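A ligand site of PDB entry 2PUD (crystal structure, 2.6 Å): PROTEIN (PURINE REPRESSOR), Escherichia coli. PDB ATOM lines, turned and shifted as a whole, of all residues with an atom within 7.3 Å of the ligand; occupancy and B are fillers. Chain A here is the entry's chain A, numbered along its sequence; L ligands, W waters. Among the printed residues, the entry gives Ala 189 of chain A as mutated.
OD2 of Asp 274 is in hydrogen-bond range of N4 of the ligand, 2.7 Å away.
N3 of the ligand lies within hydrogen-bond range of OG1 of Thr 191 (2.7 Å).
OG of Ser 123 lies within hydrogen-bond range of O1 of the ligand, at 3.4 Å.
OD1 of Asp 274 lies within salt-bridge range of NH2 of Arg 195 (2.6 Å).
N of Gln 291 is in hydrogen-bond range of O of Asp 274, at 3.1 Å.
The backbone carbonyl oxygen (O) of Thr 191 sits close to the guanidinium group (NE) of Arg 195, at 3.4 Å.
The guanidinium group (NH1) of Arg 195 sits at hydrogen-bond distance from the backbone carbonyl oxygen (O) of Gly 245.
N of Phe 220 sits at hydrogen-bond distance from SD of Met 249 (3.4 Å).
The side-chain hydroxyl (OH) of Tyr 72 is in hydrogen-bond range of the side-chain amide oxygen (OE1) of Gln 291 (3.0 Å).
The side-chain carboxylate (OD2) of Asp 145 sits at hydrogen-bond distance from the backbone NH (N) of Ser 123 (3.0 Å).
CB of Tyr 72 touches N2 of the ligand, at 3.2 Å.
Phe 73 touches the ligand (CZ to O1, 3.5 Å).
Arg 195 touches the ligand.
Phe 220 touches the ligand.
Hydrophobic or aromatic side chains within 4 Å of the ligand: Tyr 72, Phe 73 and Phe 220.
Of the 26 residues printed, 7 come within 4 Å of the ligand.
The nearest printed residue that does not touch the ligand is Ala 70 (4.5 Å).
Water W1 lies within hydrogen-bond range of a nitrogen (N2) of the ligand (3.0 Å) and the backbone NH (N) of Tyr 72 (3.1 Å).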
ATOM      1  N   THR A  66      27.974 -19.592  20.682  1.00  0.00           N
ATOM      2  CA  THR A  66      28.926 -19.494  21.768  1.00  0.00           C
ATOM      3  C   THR A  66      28.262 -19.943  23.079  1.00  0.00           C
ATOM      4  O   THR A  66      28.810 -20.737  23.815  1.00  0.00           O
ATOM      5  CB  THR A  66      29.438 -18.076  21.898  1.00  0.00           C
ATOM      6  OG1 THR A  66      30.492 -17.847  20.947  1.00  0.00           O
ATOM      7  CG2 THR A  66      29.926 -17.838  23.299  1.00  0.00           C
ATOM      8  N   ALA A  70      22.760 -16.216  27.578  1.00  0.00           N
ATOM      9  CA  ALA A  70      22.882 -14.764  27.432  1.00  0.00           C
ATOM     10  C   ALA A  70      21.765 -14.102  26.624  1.00  0.00           C
ATOM     11  O   ALA A  70      21.484 -14.475  25.465  1.00  0.00           O
ATOM     12  CB  ALA A  70      24.238 -14.404  26.848  1.00  0.00           C
ATOM     13  N   ALA A  71      21.153 -13.137  27.279  1.00  0.00           N
ATOM     14  CA  ALA A  71      20.096 -12.333  26.727  1.00  0.00           C
ATOM     15  C   ALA A  71      20.305 -12.046  25.248  1.00  0.00           C
ATOM     16  O   ALA A  71      19.491 -12.400  24.418  1.00  0.00           O
ATOM     17  CB  ALA A  71      20.020 -11.008  27.491  1.00  0.00           C
ATOM     18  N   TYR A  72      21.442 -11.416  24.981  1.00  0.00           N
ATOM     19  CA  TYR A  72      21.833 -11.004  23.647  1.00  0.00           C
ATOM     20  C   TYR A  72      21.679 -12.216  22.760  1.00  0.00           C
ATOM     21  O   TYR A  72      20.783 -12.267  21.934  1.00  0.00           O
ATOM     22  CB  TYR A  72      23.293 -10.531  23.704  1.00  0.00           C
ATOM     23  CG  TYR A  72      23.877 -10.088  22.395  1.00  0.00           C
ATOM     24  CD1 TYR A  72      23.459  -8.919  21.811  1.00  0.00           C
ATOM     25  CD2 TYR A  72      24.870 -10.808  21.771  1.00  0.00           C
ATOM     26  CE1 TYR A  72      23.986  -8.483  20.617  1.00  0.00           C
ATOM     27  CE2 TYR A  72      25.407 -10.364  20.582  1.00  0.00           C
ATOM     28  CZ  TYR A  72      24.930  -9.212  19.999  1.00  0.00           C
ATOM     29  OH  TYR A  72      25.406  -8.755  18.822  1.00  0.00           O
ATOM     30  N   PHE A  73      22.478 -13.239  23.007  1.00  0.00           N
ATOM     31  CA  PHE A  73      22.412 -14.429  22.194  1.00  0.00           C
ATOM     32  C   PHE A  73      21.066 -15.024  22.072  1.00  0.00           C
ATOM     33  O   PHE A  73      20.605 -15.414  21.000  1.00  0.00           O
ATOM     34  CB  PHE A  73      23.340 -15.486  22.759  1.00  0.00           C
ATOM     35  CG  PHE A  73      24.760 -15.127  22.591  1.00  0.00           C
ATOM     36  CD1 PHE A  73      25.198 -14.651  21.387  1.00  0.00           C
ATOM     37  CD2 PHE A  73      25.639 -15.217  23.648  1.00  0.00           C
ATOM     38  CE1 PHE A  73      26.484 -14.272  21.231  1.00  0.00           C
ATOM     39  CE2 PHE A  73      26.936 -14.835  23.505  1.00  0.00           C
ATOM     40  CZ  PHE A  73      27.362 -14.347  22.302  1.00  0.00           C
ATOM     41  N   SER A 123      31.828 -15.447  18.629  1.00  0.00           N
ATOM     42  CA  SER A 123      32.441 -14.411  19.435  1.00  0.00           C
ATOM     43  C   SER A 123      33.896 -14.198  19.100  1.00  0.00           C
ATOM     44  O   SER A 123      34.225 -13.233  18.491  1.00  0.00           O
ATOM     45  CB  SER A 123      32.264 -14.763  20.917  1.00  0.00           C
ATOM     46  OG  SER A 123      31.453 -13.819  21.583  1.00  0.00           O
ATOM     47  N   ASP A 145      28.923 -12.656  13.138  1.00  0.00           N
ATOM     48  CA  ASP A 145      29.492 -11.730  14.089  1.00  0.00           C
ATOM     49  C   ASP A 145      30.880 -11.182  13.846  1.00  0.00           C
ATOM     50  O   ASP A 145      31.613 -10.911  14.802  1.00  0.00           O
ATOM     51  CB  ASP A 145      29.330 -12.272  15.520  1.00  0.00           C
ATOM     52  CG  ASP A 145      30.044 -13.643  15.757  1.00  0.00           C
ATOM     53  OD1 ASP A 145      30.946 -14.020  14.962  1.00  0.00           O
ATOM     54  OD2 ASP A 145      29.755 -14.288  16.784  1.00  0.00           O
ATOM     55  N   ASP A 159      27.652  -5.874  11.698  1.00  0.00           N
ATOM     56  CA  ASP A 159      26.841  -5.012  12.573  1.00  0.00           C
ATOM     57  C   ASP A 159      27.182  -3.552  12.703  1.00  0.00           C
ATOM     58  O   ASP A 159      26.415  -2.834  13.252  1.00  0.00           O
ATOM     59  CB  ASP A 159      26.747  -5.625  13.954  1.00  0.00           C
ATOM     60  CG  ASP A 159      28.065  -5.641  14.640  1.00  0.00           C
ATOM     61  OD1 ASP A 159      29.074  -5.123  14.027  1.00  0.00           O
ATOM     62  OD2 ASP A 159      28.142  -6.196  15.759  1.00  0.00           O
ATOM     63  N   PRO A 186      35.127  -8.107  25.954  1.00  0.00           N
ATOM     64  CA  PRO A 186      36.391  -8.717  25.517  1.00  0.00           C
ATOM     65  C   PRO A 186      36.926  -8.152  24.228  1.00  0.00           C
ATOM     66  O   PRO A 186      36.218  -8.012  23.218  1.00  0.00           O
ATOM     67  CB  PRO A 186      36.087 -10.206  25.393  1.00  0.00           C
ATOM     68  CG  PRO A 186      34.689 -10.420  25.922  1.00  0.00           C
ATOM     69  CD  PRO A 186      34.097  -9.114  26.309  1.00  0.00           C
ATOM     70  N   ALA A 189      36.859  -9.856  20.846  1.00  0.00           N
ATOM     71  CA  ALA A 189      35.589  -9.956  20.146  1.00  0.00           C
ATOM     72  C   ALA A 189      35.199  -8.627  19.433  1.00  0.00           C
ATOM     73  O   ALA A 189      35.628  -7.546  19.825  1.00  0.00           O
ATOM     74  CB  ALA A 189      34.479 -10.462  21.098  1.00  0.00           C
ATOM     75  N   ASN A 190      34.414  -8.728  18.379  1.00  0.00           N
ATOM     76  CA  ASN A 190      34.021  -7.541  17.619  1.00  0.00           C
ATOM     77  C   ASN A 190      33.130  -6.571  18.404  1.00  0.00           C
ATOM     78  O   ASN A 190      33.422  -5.358  18.467  1.00  0.00           O
ATOM     79  CB  ASN A 190      33.338  -7.950  16.301  1.00  0.00           C
ATOM     80  CG  ASN A 190      32.724  -6.772  15.566  1.00  0.00           C
ATOM     81  OD1 ASN A 190      33.441  -5.786  15.213  1.00  0.00           O
ATOM     82  ND2 ASN A 190      31.398  -6.847  15.334  1.00  0.00           N
ATOM     83  N   THR A 191      32.046  -7.091  18.983  1.00  0.00           N
ATOM     84  CA  THR A 191      31.131  -6.276  19.781  1.00  0.00           C
ATOM     85  C   THR A 191      31.904  -5.719  20.958  1.00  0.00           C
ATOM     86  O   THR A 191      31.398  -4.852  21.663  1.00  0.00           O
ATOM     87  CB  THR A 191      30.001  -7.081  20.339  1.00  0.00           C
ATOM     88  OG1 THR A 191      30.549  -8.276  20.869  1.00  0.00           O
ATOM     89  CG2 THR A 191      28.914  -7.447  19.283  1.00  0.00           C
ATOM     90  N   GLY A 192      33.131  -6.212  21.177  1.00  0.00           N
ATOM     91  CA  GLY A 192      33.977  -5.696  22.222  1.00  0.00           C
ATOM     92  C   GLY A 192      34.889  -4.595  21.634  1.00  0.00           C
ATOM     93  O   GLY A 192      34.654  -3.413  21.772  1.00  0.00           O
ATOM     94  N   ARG A 195      33.189  -1.837  19.405  1.00  0.00           N
ATOM     95  CA  ARG A 195      32.383  -0.806  20.061  1.00  0.00           C
ATOM     96  C   ARG A 195      33.299   0.183  20.773  1.00  0.00           C
ATOM     97  O   ARG A 195      33.139   1.383  20.722  1.00  0.00           O
ATOM     98  CB  ARG A 195      31.291  -1.433  20.988  1.00  0.00           C
ATOM     99  CG  ARG A 195      30.317  -2.440  20.277  1.00  0.00           C
ATOM    100  CD  ARG A 195      29.244  -3.039  21.235  1.00  0.00           C
ATOM    101  NE  ARG A 195      28.270  -3.890  20.571  1.00  0.00           N
ATOM    102  CZ  ARG A 195      27.454  -4.714  21.240  1.00  0.00           C
ATOM    103  NH1 ARG A 195      27.561  -4.764  22.550  1.00  0.00           N
ATOM    104  NH2 ARG A 195      26.557  -5.496  20.624  1.00  0.00           N
ATOM    105  N   ASP A 219      33.142  -8.770  30.520  1.00  0.00           N
ATOM    106  CA  ASP A 219      33.079 -10.038  29.787  1.00  0.00           C
ATOM    107  C   ASP A 219      31.662 -10.262  29.368  1.00  0.00           C
ATOM    108  O   ASP A 219      31.278 -11.371  29.125  1.00  0.00           O
ATOM    109  CB  ASP A 219      33.582 -11.196  30.647  1.00  0.00           C
ATOM    110  CG  ASP A 219      32.796 -11.376  31.921  1.00  0.00           C
ATOM    111  OD1 ASP A 219      31.635 -10.932  32.065  1.00  0.00           O
ATOM    112  OD2 ASP A 219      33.350 -12.032  32.805  1.00  0.00           O
ATOM    113  N   PHE A 220      30.888  -9.173  29.326  1.00  0.00           N
ATOM    114  CA  PHE A 220      29.451  -9.212  28.996  1.00  0.00           C
ATOM    115  C   PHE A 220      28.567  -9.776  30.115  1.00  0.00           C
ATOM    116  O   PHE A 220      27.361  -9.714  30.041  1.00  0.00           O
ATOM    117  CB  PHE A 220      29.155  -9.944  27.721  1.00  0.00           C
ATOM    118  CG  PHE A 220      29.637  -9.235  26.537  1.00  0.00           C
ATOM    119  CD1 PHE A 220      29.154  -8.007  26.240  1.00  0.00           C
ATOM    120  CD2 PHE A 220      30.629  -9.791  25.730  1.00  0.00           C
ATOM    121  CE1 PHE A 220      29.591  -7.328  25.136  1.00  0.00           C
ATOM    122  CE2 PHE A 220      31.090  -9.120  24.638  1.00  0.00           C
ATOM    123  CZ  PHE A 220      30.551  -7.867  24.338  1.00  0.00           C
ATOM    124  N   GLU A 221      29.165 -10.340  31.142  1.00  0.00           N
ATOM    125  CA  GLU A 221      28.386 -10.872  32.246  1.00  0.00           C
ATOM    126  C   GLU A 221      28.159  -9.790  33.340  1.00  0.00           C
ATOM    127  O   GLU A 221      29.012  -8.929  33.637  1.00  0.00           O
ATOM    128  CB  GLU A 221      29.099 -12.097  32.825  1.00  0.00           C
ATOM    129  CG  GLU A 221      29.133 -13.301  31.896  1.00  0.00           C
ATOM    130  CD  GLU A 221      27.887 -14.163  32.043  1.00  0.00           C
ATOM    131  OE1 GLU A 221      26.803 -13.707  31.612  1.00  0.00           O
ATOM    132  OE2 GLU A 221      27.999 -15.274  32.626  1.00  0.00           O
ATOM    133  N   GLY A 245      29.842  -1.385  27.470  1.00  0.00           N
ATOM    134  CA  GLY A 245      29.785  -2.203  26.272  1.00  0.00           C
ATOM    135  C   GLY A 245      28.613  -3.148  26.005  1.00  0.00           C
ATOM    136  O   GLY A 245      28.499  -3.664  24.923  1.00  0.00           O
ATOM    137  N   GLY A 246      27.749  -3.398  26.980  1.00  0.00           N
ATOM    138  CA  GLY A 246      26.644  -4.315  26.796  1.00  0.00           C
ATOM    139  C   GLY A 246      25.611  -4.137  27.900  1.00  0.00           C
ATOM    140  O   GLY A 246      25.942  -3.870  29.065  1.00  0.00           O
ATOM    141  N   ASP A 247      24.337  -4.299  27.558  1.00  0.00           N
ATOM    142  CA  ASP A 247      23.320  -4.062  28.546  1.00  0.00           C
ATOM    143  C   ASP A 247      23.407  -4.894  29.860  1.00  0.00           C
ATOM    144  O   ASP A 247      23.358  -4.355  30.979  1.00  0.00           O
ATOM    145  CB  ASP A 247      21.971  -4.160  27.869  1.00  0.00           C
ATOM    146  CG  ASP A 247      21.693  -2.996  26.941  1.00  0.00           C
ATOM    147  OD1 ASP A 247      22.529  -2.078  26.868  1.00  0.00           O
ATOM    148  OD2 ASP A 247      20.653  -3.011  26.235  1.00  0.00           O
ATOM    149  N   ILE A 248      23.502  -6.209  29.730  1.00  0.00           N
ATOM    150  CA  ILE A 248      23.579  -7.035  30.894  1.00  0.00           C
ATOM    151  C   ILE A 248      24.732  -6.627  31.809  1.00  0.00           C
ATOM    152  O   ILE A 248      24.613  -6.675  33.037  1.00  0.00           O
ATOM    153  CB  ILE A 248      23.655  -8.525  30.549  1.00  0.00           C
ATOM    154  CG1 ILE A 248      22.506  -8.921  29.604  1.00  0.00           C
ATOM    155  CG2 ILE A 248      23.744  -9.395  31.831  1.00  0.00           C
ATOM    156  CD1 ILE A 248      21.172  -8.856  30.210  1.00  0.00           C
ATOM    157  N   MET A 249      25.843  -6.194  31.244  1.00  0.00           N
ATOM    158  CA  MET A 249      26.935  -5.750  32.126  1.00  0.00           C
ATOM    159  C   MET A 249      26.403  -4.425  32.761  1.00  0.00           C
ATOM    160  O   MET A 249      26.660  -4.110  33.893  1.00  0.00           O
ATOM    161  CB  MET A 249      28.191  -5.400  31.311  1.00  0.00           C
ATOM    162  CG  MET A 249      29.134  -6.516  30.958  1.00  0.00           C
ATOM    163  SD  MET A 249      30.802  -5.939  30.387  1.00  0.00           S
ATOM    164  CE  MET A 249      30.461  -5.051  28.845  1.00  0.00           C
ATOM    165  N   TYR A 273      24.560  -0.823  25.646  1.00  0.00           N
ATOM    166  CA  TYR A 273      24.594  -1.230  24.270  1.00  0.00           C
ATOM    167  C   TYR A 273      23.996  -2.572  24.120  1.00  0.00           C
ATOM    168  O   TYR A 273      24.433  -3.469  24.815  1.00  0.00           O
ATOM    169  CB  TYR A 273      26.039  -1.380  23.854  1.00  0.00           C
ATOM    170  CG  TYR A 273      26.209  -1.288  22.372  1.00  0.00           C
ATOM    171  CD1 TYR A 273      25.492  -2.109  21.519  1.00  0.00           C
ATOM    172  CD2 TYR A 273      27.080  -0.343  21.813  1.00  0.00           C
ATOM    173  CE1 TYR A 273      25.691  -2.047  20.138  1.00  0.00           C
ATOM    174  CE2 TYR A 273      27.278  -0.257  20.451  1.00  0.00           C
ATOM    175  CZ  TYR A 273      26.579  -1.117  19.614  1.00  0.00           C
ATOM    176  OH  TYR A 273      26.791  -0.992  18.253  1.00  0.00           O
ATOM    177  N   ASP A 274      23.029  -2.677  23.229  1.00  0.00           N
ATOM    178  CA  ASP A 274      22.330  -3.891  22.790  1.00  0.00           C
ATOM    179  C   ASP A 274      20.858  -3.687  22.665  1.00  0.00           C
ATOM    180  O   ASP A 274      20.197  -4.131  21.721  1.00  0.00           O
ATOM    181  CB  ASP A 274      22.613  -5.132  23.654  1.00  0.00           C
ATOM    182  CG  ASP A 274      23.993  -5.781  23.352  1.00  0.00           C
ATOM    183  OD1 ASP A 274      24.704  -5.350  22.380  1.00  0.00           O
ATOM    184  OD2 ASP A 274      24.363  -6.680  24.154  1.00  0.00           O
ATOM    185  N   VAL A 276      18.662  -4.920  24.777  1.00  0.00           N
ATOM    186  CA  VAL A 276      18.125  -6.249  24.962  1.00  0.00           C
ATOM    187  C   VAL A 276      16.675  -6.113  25.394  1.00  0.00           C
ATOM    188  O   VAL A 276      16.329  -5.233  26.172  1.00  0.00           O
ATOM    189  CB  VAL A 276      19.016  -6.901  26.009  1.00  0.00           C
ATOM    190  CG1 VAL A 276      18.324  -7.208  27.287  1.00  0.00           C
ATOM    191  CG2 VAL A 276      19.911  -7.967  25.434  1.00  0.00           C
ATOM    192  N   GLN A 291      20.843  -2.910  18.924  1.00  0.00           N
ATOM    193  CA  GLN A 291      21.393  -3.789  17.908  1.00  0.00           C
ATOM    194  C   GLN A 291      20.195  -4.473  17.308  1.00  0.00           C
ATOM    195  O   GLN A 291      19.281  -4.928  18.025  1.00  0.00           O
ATOM    196  CB  GLN A 291      22.280  -4.871  18.516  1.00  0.00           C
ATOM    197  CG  GLN A 291      22.801  -5.887  17.490  1.00  0.00           C
ATOM    198  CD  GLN A 291      24.213  -5.527  16.943  1.00  0.00           C
ATOM    199  OE1 GLN A 291      25.205  -6.201  17.237  1.00  0.00           O
ATOM    200  NE2 GLN A 291      24.279  -4.459  16.174  1.00  0.00           N
HETATM  201  N1  LIG L   1      27.798 -11.482  24.778  1.00  0.00           N
HETATM  202  C1  LIG L   1      26.713 -10.896  25.384  1.00  0.00           C
HETATM  203  N2  LIG L   1      26.170  -9.754  24.982  1.00  0.00           N
HETATM  204  C2  LIG L   1      26.801  -9.239  23.903  1.00  0.00           C
HETATM  205  C3  LIG L   1      27.875  -9.754  23.225  1.00  0.00           C
HETATM  206  C4  LIG L   1      28.457 -10.971  23.675  1.00  0.00           C
HETATM  207  O1  LIG L   1      29.405 -11.606  23.211  1.00  0.00           O
HETATM  208  N3  LIG L   1      28.252  -8.897  22.215  1.00  0.00           N
HETATM  209  C5  LIG L   1      27.396  -7.915  22.266  1.00  0.00           C
HETATM  210  N4  LIG L   1      26.478  -8.063  23.272  1.00  0.00           N
HETATM  211  O   HOH W   1      23.938 -10.901  26.687  1.00  0.00           O
